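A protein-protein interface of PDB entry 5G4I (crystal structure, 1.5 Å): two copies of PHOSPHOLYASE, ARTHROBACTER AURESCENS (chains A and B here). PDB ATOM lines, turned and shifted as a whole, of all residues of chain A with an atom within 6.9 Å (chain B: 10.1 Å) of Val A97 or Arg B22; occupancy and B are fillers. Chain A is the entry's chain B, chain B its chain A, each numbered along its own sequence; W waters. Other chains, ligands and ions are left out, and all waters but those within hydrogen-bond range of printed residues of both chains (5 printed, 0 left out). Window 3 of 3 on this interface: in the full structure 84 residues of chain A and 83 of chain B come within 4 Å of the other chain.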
ATOM      1  N   LEU A  92      18.821 -13.995   4.217  1.00  0.00           N
ATOM      2  CA  LEU A  92      18.500 -12.946   3.279  1.00  0.00           C
ATOM      3  C   LEU A  92      19.458 -11.762   3.384  1.00  0.00           C
ATOM      4  O   LEU A  92      19.967 -11.423   4.495  1.00  0.00           O
ATOM      5  CB  LEU A  92      17.056 -12.377   3.581  1.00  0.00           C
ATOM      6  CG  LEU A  92      15.895 -13.321   3.306  1.00  0.00           C
ATOM      7  CD1 LEU A  92      14.607 -12.643   3.841  1.00  0.00           C
ATOM      8  CD2 LEU A  92      15.739 -13.626   1.802  1.00  0.00           C
ATOM      9  N   ASN A  93      19.692 -11.131   2.231  1.00  0.00           N
ATOM     10  CA  ASN A  93      20.516  -9.935   2.150  1.00  0.00           C
ATOM     11  C   ASN A  93      20.214  -9.222   0.798  1.00  0.00           C
ATOM     12  O   ASN A  93      19.984  -9.888  -0.213  1.00  0.00           O
ATOM     13  CB  ASN A  93      22.040 -10.215   2.350  1.00  0.00           C
ATOM     14  CG  ASN A  93      22.898  -8.965   2.412  1.00  0.00           C
ATOM     15  OD1 ASN A  93      23.201  -8.390   3.531  1.00  0.00           O
ATOM     16  ND2 ASN A  93      23.290  -8.481   1.269  1.00  0.00           N
ATOM     17  N   SER A  94      20.128  -7.885   0.824  1.00  0.00           N
ATOM     18  CA  SER A  94      19.636  -7.158  -0.357  1.00  0.00           C
ATOM     19  C   SER A  94      20.569  -7.147  -1.563  1.00  0.00           C
ATOM     20  O   SER A  94      20.097  -7.029  -2.684  1.00  0.00           O
ATOM     21  CB  SER A  94      19.209  -5.739   0.024  1.00  0.00           C
ATOM     22  OG  SER A  94      20.330  -4.937   0.310  1.00  0.00           O
ATOM     23  N   ARG A  95      21.879  -7.267  -1.321  1.00  0.00           N
ATOM     24  CA  ARG A  95      22.833  -7.053  -2.444  1.00  0.00           C
ATOM     25  C   ARG A  95      22.663  -8.042  -3.621  1.00  0.00           C
ATOM     26  O   ARG A  95      22.626  -7.640  -4.755  1.00  0.00           O
ATOM     27  CB  ARG A  95      24.303  -6.967  -2.003  1.00  0.00           C
ATOM     28  CG  ARG A  95      24.643  -6.063  -0.822  1.00  0.00           C
ATOM     29  CD  ARG A  95      24.179  -4.583  -0.913  1.00  0.00           C
ATOM     30  NE  ARG A  95      24.566  -3.981  -2.147  1.00  0.00           N
ATOM     31  CZ  ARG A  95      25.740  -3.376  -2.397  1.00  0.00           C
ATOM     32  NH1 ARG A  95      26.720  -3.442  -1.534  1.00  0.00           N
ATOM     33  NH2 ARG A  95      25.971  -2.722  -3.574  1.00  0.00           N
ATOM     34  N   VAL A  96      22.530  -9.341  -3.289  1.00  0.00           N
ATOM     35  CA  VAL A  96      22.322 -10.357  -4.300  1.00  0.00           C
ATOM     36  C   VAL A  96      21.006 -10.185  -5.106  1.00  0.00           C
ATOM     37  O   VAL A  96      20.980 -10.383  -6.328  1.00  0.00           O
ATOM     38  CB  VAL A  96      22.451 -11.805  -3.769  1.00  0.00           C
ATOM     39  CG1 VAL A  96      21.334 -12.131  -2.777  1.00  0.00           C
ATOM     40  CG2 VAL A  96      22.534 -12.849  -4.914  1.00  0.00           C
ATOM     41  N   VAL A  97      19.967  -9.724  -4.417  1.00  0.00           N
ATOM     42  CA  VAL A  97      18.721  -9.445  -5.129  1.00  0.00           C
ATOM     43  C   VAL A  97      18.789  -8.214  -6.048  1.00  0.00           C
ATOM     44  O   VAL A  97      18.325  -8.249  -7.199  1.00  0.00           O
ATOM     45  CB  VAL A  97      17.580  -9.320  -4.058  1.00  0.00           C
ATOM     46  CG1 VAL A  97      16.236  -8.990  -4.769  1.00  0.00           C
ATOM     47  CG2 VAL A  97      17.414 -10.621  -3.288  1.00  0.00           C
ATOM     48  N   GLU A  98      19.425  -7.154  -5.541  1.00  0.00           N
ATOM     49  CA  GLU A  98      19.735  -6.002  -6.400  1.00  0.00           C
ATOM     50  C   GLU A  98      20.533  -6.353  -7.643  1.00  0.00           C
ATOM     51  O   GLU A  98      20.233  -5.889  -8.755  1.00  0.00           O
ATOM     52  CB  GLU A  98      20.443  -4.916  -5.625  1.00  0.00           C
ATOM     53  CG  GLU A  98      19.647  -4.276  -4.488  1.00  0.00           C
ATOM     54  CD  GLU A  98      20.507  -3.637  -3.359  1.00  0.00           C
ATOM     55  OE1 GLU A  98      21.772  -3.436  -3.507  1.00  0.00           O
ATOM     56  OE2 GLU A  98      19.873  -3.286  -2.314  1.00  0.00           O
ATOM     57  N   TYR A  99      21.597  -7.172  -7.456  1.00  0.00           N
ATOM     58  CA  TYR A  99      22.376  -7.566  -8.591  1.00  0.00           C
ATOM     59  C   TYR A  99      21.564  -8.431  -9.557  1.00  0.00           C
ATOM     60  O   TYR A  99      21.677  -8.220 -10.766  1.00  0.00           O
ATOM     61  CB  TYR A  99      23.676  -8.271  -8.147  1.00  0.00           C
ATOM     62  CG  TYR A  99      24.580  -8.677  -9.306  1.00  0.00           C
ATOM     63  CD1 TYR A  99      24.869  -7.828 -10.322  1.00  0.00           C
ATOM     64  CD2 TYR A  99      25.111  -9.927  -9.330  1.00  0.00           C
ATOM     65  CE1 TYR A  99      25.709  -8.165 -11.400  1.00  0.00           C
ATOM     66  CE2 TYR A  99      25.965 -10.315 -10.414  1.00  0.00           C
ATOM     67  CZ  TYR A  99      26.239  -9.444 -11.405  1.00  0.00           C
ATOM     68  OH  TYR A  99      27.092  -9.771 -12.494  1.00  0.00           O
ATOM     69  N   ALA A 100      20.810  -9.389  -9.050  1.00  0.00           N
ATOM     70  CA  ALA A 100      20.001 -10.290  -9.910  1.00  0.00           C
ATOM     71  C   ALA A 100      19.013  -9.468 -10.753  1.00  0.00           C
ATOM     72  O   ALA A 100      18.876  -9.682 -11.957  1.00  0.00           O
ATOM     73  CB  ALA A 100      19.280 -11.354  -9.082  1.00  0.00           C
ATOM     74  N   GLU A 101      18.406  -8.484 -10.113  1.00  0.00           N
ATOM     75  CA  GLU A 101      17.479  -7.579 -10.849  1.00  0.00           C
ATOM     76  C   GLU A 101      18.154  -6.770 -11.953  1.00  0.00           C
ATOM     77  O   GLU A 101      17.683  -6.695 -13.113  1.00  0.00           O
ATOM     78  CB  GLU A 101      16.767  -6.642  -9.859  1.00  0.00           C
ATOM     79  CG  GLU A 101      15.724  -7.368  -9.022  1.00  0.00           C
ATOM     80  CD  GLU A 101      15.140  -6.532  -7.877  1.00  0.00           C
ATOM     81  OE1 GLU A 101      15.761  -5.555  -7.380  1.00  0.00           O
ATOM     82  OE2 GLU A 101      14.091  -6.981  -7.337  1.00  0.00           O
ATOM     83  N   ALA A 102      19.357  -6.266 -11.649  1.00  0.00           N
ATOM     84  CA  ALA A 102      20.127  -5.478 -12.624  1.00  0.00           C
ATOM     85  C   ALA A 102      20.544  -6.347 -13.802  1.00  0.00           C
ATOM     86  O   ALA A 102      20.460  -5.968 -14.990  1.00  0.00           O
ATOM     87  CB  ALA A 102      21.338  -4.801 -11.950  1.00  0.00           C
ATOM     88  N   GLY A 314      26.829 -15.652  -5.045  1.00  0.00           N
ATOM     89  CA  GLY A 314      25.801 -14.681  -4.565  1.00  0.00           C
ATOM     90  C   GLY A 314      26.044 -14.088  -3.207  1.00  0.00           C
ATOM     91  O   GLY A 314      25.124 -13.542  -2.546  1.00  0.00           O
ATOM     92  N   SER A 319      28.324  -9.818  -5.216  1.00  0.00           N
ATOM     93  CA  SER A 319      27.174  -9.072  -5.773  1.00  0.00           C
ATOM     94  C   SER A 319      27.464  -7.558  -5.913  1.00  0.00           C
ATOM     95  O   SER A 319      27.106  -6.980  -6.946  1.00  0.00           O
ATOM     96  CB  SER A 319      25.966  -9.283  -4.868  1.00  0.00           C
ATOM     97  OG  SER A 319      25.561 -10.689  -4.788  1.00  0.00           O
ATOM     98  N   LEU A 323      27.484  -5.534  -9.477  1.00  0.00           N
ATOM     99  CA  LEU A 323      26.598  -4.333  -9.622  1.00  0.00           C
ATOM    100  C   LEU A 323      27.468  -3.140 -10.075  1.00  0.00           C
ATOM    101  O   LEU A 323      27.015  -2.332 -10.968  1.00  0.00           O
ATOM    102  CB  LEU A 323      25.912  -4.009  -8.310  1.00  0.00           C
ATOM    103  CG  LEU A 323      24.586  -4.676  -7.972  1.00  0.00           C
ATOM    104  CD1 LEU A 323      24.347  -4.583  -6.417  1.00  0.00           C
ATOM    105  CD2 LEU A 323      23.469  -3.986  -8.831  1.00  0.00           C
ATOM    106  N   ASP B  18       9.187  -6.799   1.084  1.00  0.00           N
ATOM    107  CA  ASP B  18       9.317  -7.093  -0.322  1.00  0.00           C
ATOM    108  C   ASP B  18      10.544  -7.951  -0.621  1.00  0.00           C
ATOM    109  O   ASP B  18      10.526  -8.501  -1.694  1.00  0.00           O
ATOM    110  CB  ASP B  18       9.488  -5.746  -1.079  1.00  0.00           C
ATOM    111  CG  ASP B  18      10.713  -4.935  -0.531  1.00  0.00           C
ATOM    112  OD1 ASP B  18      10.506  -4.355   0.543  1.00  0.00           O
ATOM    113  OD2 ASP B  18      11.861  -4.927  -1.051  1.00  0.00           O
ATOM    114  N   LEU B  19      11.581  -7.986   0.240  1.00  0.00           N
ATOM    115  CA  LEU B  19      12.860  -8.708  -0.161  1.00  0.00           C
ATOM    116  C   LEU B  19      12.634 -10.176  -0.492  1.00  0.00           C
ATOM    117  O   LEU B  19      13.217 -10.690  -1.513  1.00  0.00           O
ATOM    118  CB  LEU B  19      13.931  -8.497   0.898  1.00  0.00           C
ATOM    119  CG  LEU B  19      15.322  -8.992   0.502  1.00  0.00           C
ATOM    120  CD1 LEU B  19      15.780  -8.234  -0.753  1.00  0.00           C
ATOM    121  CD2 LEU B  19      16.325  -8.771   1.635  1.00  0.00           C
ATOM    122  N   LEU B  20      11.894 -10.928   0.339  1.00  0.00           N
ATOM    123  CA  LEU B  20      11.696 -12.349   0.097  1.00  0.00           C
ATOM    124  C   LEU B  20      11.019 -12.631  -1.269  1.00  0.00           C
ATOM    125  O   LEU B  20      11.442 -13.465  -2.094  1.00  0.00           O
ATOM    126  CB  LEU B  20      10.874 -12.989   1.241  1.00  0.00           C
ATOM    127  CG  LEU B  20      10.719 -14.487   1.211  1.00  0.00           C
ATOM    128  CD1 LEU B  20      12.021 -15.299   1.338  1.00  0.00           C
ATOM    129  CD2 LEU B  20       9.808 -14.961   2.366  1.00  0.00           C
ATOM    130  N   ALA B  21       9.943 -11.848  -1.570  1.00  0.00           N
ATOM    131  CA  ALA B  21       9.301 -12.008  -2.858  1.00  0.00           C
ATOM    132  C   ALA B  21      10.215 -11.626  -4.059  1.00  0.00           C
ATOM    133  O   ALA B  21      10.193 -12.334  -5.093  1.00  0.00           O
ATOM    134  CB  ALA B  21       7.996 -11.165  -2.905  1.00  0.00           C
ATOM    135  N   ARG B  22      11.012 -10.563  -3.882  1.00  0.00           N
ATOM    136  CA  ARG B  22      11.965 -10.114  -4.917  1.00  0.00           C
ATOM    137  C   ARG B  22      13.039 -11.230  -5.185  1.00  0.00           C
ATOM    138  O   ARG B  22      13.401 -11.493  -6.353  1.00  0.00           O
ATOM    139  CB  ARG B  22      12.629  -8.826  -4.611  1.00  0.00           C
ATOM    140  CG  ARG B  22      11.639  -7.606  -4.643  1.00  0.00           C
ATOM    141  CD  ARG B  22      12.205  -6.353  -4.041  1.00  0.00           C
ATOM    142  NE  ARG B  22      13.507  -5.969  -4.625  1.00  0.00           N
ATOM    143  CZ  ARG B  22      14.486  -5.308  -3.978  1.00  0.00           C
ATOM    144  NH1 ARG B  22      14.361  -4.862  -2.692  1.00  0.00           N
ATOM    145  NH2 ARG B  22      15.622  -5.070  -4.627  1.00  0.00           N
ATOM    146  N   ARG B  23      13.460 -11.887  -4.118  1.00  0.00           N
ATOM    147  CA  ARG B  23      14.334 -13.081  -4.242  1.00  0.00           C
ATOM    148  C   ARG B  23      13.733 -14.206  -4.999  1.00  0.00           C
ATOM    149  O   ARG B  23      14.322 -14.823  -5.937  1.00  0.00           O
ATOM    150  CB  ARG B  23      14.777 -13.515  -2.828  1.00  0.00           C
ATOM    151  CG  ARG B  23      15.660 -14.774  -2.828  1.00  0.00           C
ATOM    152  CD  ARG B  23      15.856 -15.244  -1.445  1.00  0.00           C
ATOM    153  NE  ARG B  23      16.516 -16.573  -1.333  1.00  0.00           N
ATOM    154  CZ  ARG B  23      17.750 -16.825  -0.782  1.00  0.00           C
ATOM    155  NH1 ARG B  23      18.525 -15.823  -0.370  1.00  0.00           N
ATOM    156  NH2 ARG B  23      18.143 -18.134  -0.680  1.00  0.00           N
ATOM    157  N   TYR B  24      12.505 -14.574  -4.653  1.00  0.00           N
ATOM    158  CA  TYR B  24      11.858 -15.709  -5.291  1.00  0.00           C
ATOM    159  C   TYR B  24      11.601 -15.470  -6.791  1.00  0.00           C
ATOM    160  O   TYR B  24      11.589 -16.430  -7.571  1.00  0.00           O
ATOM    161  CB  TYR B  24      10.540 -16.056  -4.547  1.00  0.00           C
ATOM    162  CG  TYR B  24      10.648 -16.724  -3.218  1.00  0.00           C
ATOM    163  CD1 TYR B  24      11.870 -17.109  -2.638  1.00  0.00           C
ATOM    164  CD2 TYR B  24       9.496 -16.943  -2.439  1.00  0.00           C
ATOM    165  CE1 TYR B  24      11.955 -17.726  -1.375  1.00  0.00           C
ATOM    166  CE2 TYR B  24       9.599 -17.534  -1.178  1.00  0.00           C
ATOM    167  CZ  TYR B  24      10.809 -17.976  -0.679  1.00  0.00           C
ATOM    168  OH  TYR B  24      10.912 -18.583   0.608  1.00  0.00           O
ATOM    169  N   ALA B  25      11.442 -14.197  -7.204  1.00  0.00           N
ATOM    170  CA  ALA B  25      11.233 -13.819  -8.581  1.00  0.00           C
ATOM    171  C   ALA B  25      12.504 -13.782  -9.434  1.00  0.00           C
ATOM    172  O   ALA B  25      12.444 -13.528 -10.649  1.00  0.00           O
ATOM    173  CB  ALA B  25      10.538 -12.442  -8.666  1.00  0.00           C
ATOM    174  N   THR B  26      13.690 -13.999  -8.804  1.00  0.00           N
ATOM    175  CA  THR B  26      14.972 -13.842  -9.535  1.00  0.00           C
ATOM    176  C   THR B  26      15.857 -15.100  -9.385  1.00  0.00           C
ATOM    177  O   THR B  26      16.137 -15.809 -10.407  1.00  0.00           O
ATOM    178  CB  THR B  26      15.748 -12.578  -9.036  1.00  0.00           C
ATOM    179  OG1 THR B  26      15.874 -12.542  -7.594  1.00  0.00           O
ATOM    180  CG2 THR B  26      15.121 -11.245  -9.532  1.00  0.00           C
ATOM    181  N   ILE B  27      16.250 -15.418  -8.170  1.00  0.00           N
ATOM    182  CA  ILE B  27      17.031 -16.657  -7.931  1.00  0.00           C
ATOM    183  C   ILE B  27      16.165 -17.852  -7.489  1.00  0.00           C
ATOM    184  O   ILE B  27      16.644 -18.990  -7.368  1.00  0.00           O
ATOM    185  CB  ILE B  27      18.181 -16.443  -6.947  1.00  0.00           C
ATOM    186  CG1 ILE B  27      17.695 -16.038  -5.599  1.00  0.00           C
ATOM    187  CG2 ILE B  27      19.193 -15.453  -7.523  1.00  0.00           C
ATOM    188  CD1 ILE B  27      18.814 -16.080  -4.489  1.00  0.00           C
ATOM    189  N   GLY B  28      14.846 -17.622  -7.341  1.00  0.00           N
ATOM    190  CA  GLY B  28      13.855 -18.721  -7.164  1.00  0.00           C
ATOM    191  C   GLY B  28      13.589 -19.077  -5.744  1.00  0.00           C
ATOM    192  O   GLY B  28      14.324 -18.685  -4.849  1.00  0.00           O
ATOM    193  N   PRO B  29      12.544 -19.878  -5.506  1.00  0.00           N
ATOM    194  CA  PRO B  29      12.113 -20.255  -4.180  1.00  0.00           C
ATOM    195  C   PRO B  29      12.750 -21.563  -3.651  1.00  0.00           C
ATOM    196  O   PRO B  29      12.540 -21.936  -2.464  1.00  0.00           O
ATOM    197  CB  PRO B  29      10.591 -20.523  -4.413  1.00  0.00           C
ATOM    198  CG  PRO B  29      10.529 -21.099  -5.752  1.00  0.00           C
ATOM    199  CD  PRO B  29      11.619 -20.405  -6.559  1.00  0.00           C
ATOM    200  N   LEU B  33      16.961 -21.400   2.521  1.00  0.00           N
ATOM    201  CA  LEU B  33      16.992 -20.403   3.576  1.00  0.00           C
ATOM    202  C   LEU B  33      16.824 -21.054   4.934  1.00  0.00           C
ATOM    203  O   LEU B  33      15.993 -21.993   5.107  1.00  0.00           O
ATOM    204  CB  LEU B  33      15.833 -19.371   3.433  1.00  0.00           C
ATOM    205  CG  LEU B  33      15.963 -18.388   2.266  1.00  0.00           C
ATOM    206  CD1 LEU B  33      14.652 -17.650   1.948  1.00  0.00           C
ATOM    207  CD2 LEU B  33      17.053 -17.345   2.633  1.00  0.00           C
ATOM    208  N   GLU B  40      17.048 -11.707   7.744  1.00  0.00           N
ATOM    209  CA  GLU B  40      17.768 -10.758   6.924  1.00  0.00           C
ATOM    210  C   GLU B  40      18.911 -10.197   7.757  1.00  0.00           C
ATOM    211  O   GLU B  40      18.718  -9.416   8.712  1.00  0.00           O
ATOM    212  CB  GLU B  40      16.868  -9.591   6.394  1.00  0.00           C
ATOM    213  CG  GLU B  40      17.601  -8.639   5.475  1.00  0.00           C
ATOM    214  CD  GLU B  40      16.766  -7.485   4.931  1.00  0.00           C
ATOM    215  OE1 GLU B  40      15.542  -7.555   5.174  1.00  0.00           O
ATOM    216  OE2 GLU B  40      17.363  -6.508   4.415  1.00  0.00           O
HETATM  217  O   HOH W   1      19.996  -6.586   3.425  1.00  0.00           O
HETATM  218  O   HOH W   2      12.694  -9.189  -8.026  1.00  0.00           O
HETATM  219  O   HOH W   3      16.983  -3.053  -2.556  1.00  0.00           O
HETATM  220  O   HOH W   4      21.122 -13.742   0.457  1.00  0.00           O
HETATM  221  O   HOH W   5      18.706 -12.811  -0.370  1.00  0.00           O
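The guanidinium group (NH2) of Arg B22 lies within salt-bridge range of the side-chain carboxylate (OE1) of Glu A101 (2.8 Å).
The backbone carbonyl oxygen of Arg B23 is in hydrogen-bond range of the backbone NH of Gly B28.
O of Arg B23 is in hydrogen-bond range of OG1 of Thr B26.
OG of Ser A94 sits at hydrogen-bond distance from OE2 of Glu A98 (3.1 Å).
The side-chain hydroxyl (OG1) of Thr B26 lies within hydrogen-bond range of the backbone carbonyl oxygen (O) of Arg B22 (3.0 Å).
The side-chain carboxylate of Asp B18 lies within salt-bridge range of the guanidinium group of Arg B22 (3.0 Å).
Leu A92 touches Arg B23 (CD2 to CD, 3.6 Å).
Leu A92 touches Glu B40.
Ser A94 touches Leu B19 (N to CD2, 3.99 Å).
Leu B19 touches Val A97.
Val A97 touches Arg B22.
Val A97 touches Arg B23.
Thr B26 touches Ala A100.
Glu A101 touches Thr B26 (CG to CG2, 3.96 Å).
Of chain B, only Leu B19, Arg B22 and Arg B23 come within 4 Å of Val A97.
Arg B22 touches just these residues of chain A: Val A97 and Glu A101.
No residue of chain B comes within 4 Å of Val A96.
Ala A100 touches just one residue of chain B: Thr B26 (3.7 Å).
Of the printed residues of chain B, Ser A94 touches Leu B19 (3.99 Å).
Printed residues of chain B within 4 Å of Leu A92: Arg B23 and Glu B40.
Printed residues of chain A within 4 Å of Leu B19: Ser A94 (3.99 Å) and Val A97 (3.8 Å).
Printed residues of chain B within 4 Å of Glu A101: Arg B22 and Thr B26.
Gly B28 touches none of the printed residues of chain A.
The nearest residue of chain A that does not touch Arg B22 is Glu A98 (4.1 Å).
Of the 14 printed residues of chain B, 5 touch a printed residue of chain A.
Hydrophobic or aromatic side chains of chain B that line the printed part of chain A: Leu B19.
Hydrophobic or aromatic side chains of chain A within 4 Å of the printed part of chain B: Leu A92, Val A97 and Ala A100.
No position is printed for both chains.
Of the 9 pairs that touch across the chains among the printed residues, none has its exchanged pair printed and touching as well.
Water W2 lies within hydrogen-bond range of OE2 of Glu A101 (2.7 Å) and O of Arg B22 (2.9 Å).
Water W1 bridges OE2 of Glu B40 (2.8 Å) and N of Ser A94 (2.9 Å).
Water W3 lies within hydrogen-bond range of OE2 of Glu A98 (2.9 Å) and NH1 of Arg B22 (3.2 Å).
Water W5 lies within hydrogen-bond range of NH1 of Arg B23 (3.0 Å) and O of Asn A93 (3.2 Å).
Water W4 lies within hydrogen-bond range of the guanidinium group of Arg B23 (3.4 Å) and the backbone NH of Asn A93 (3.5 Å).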
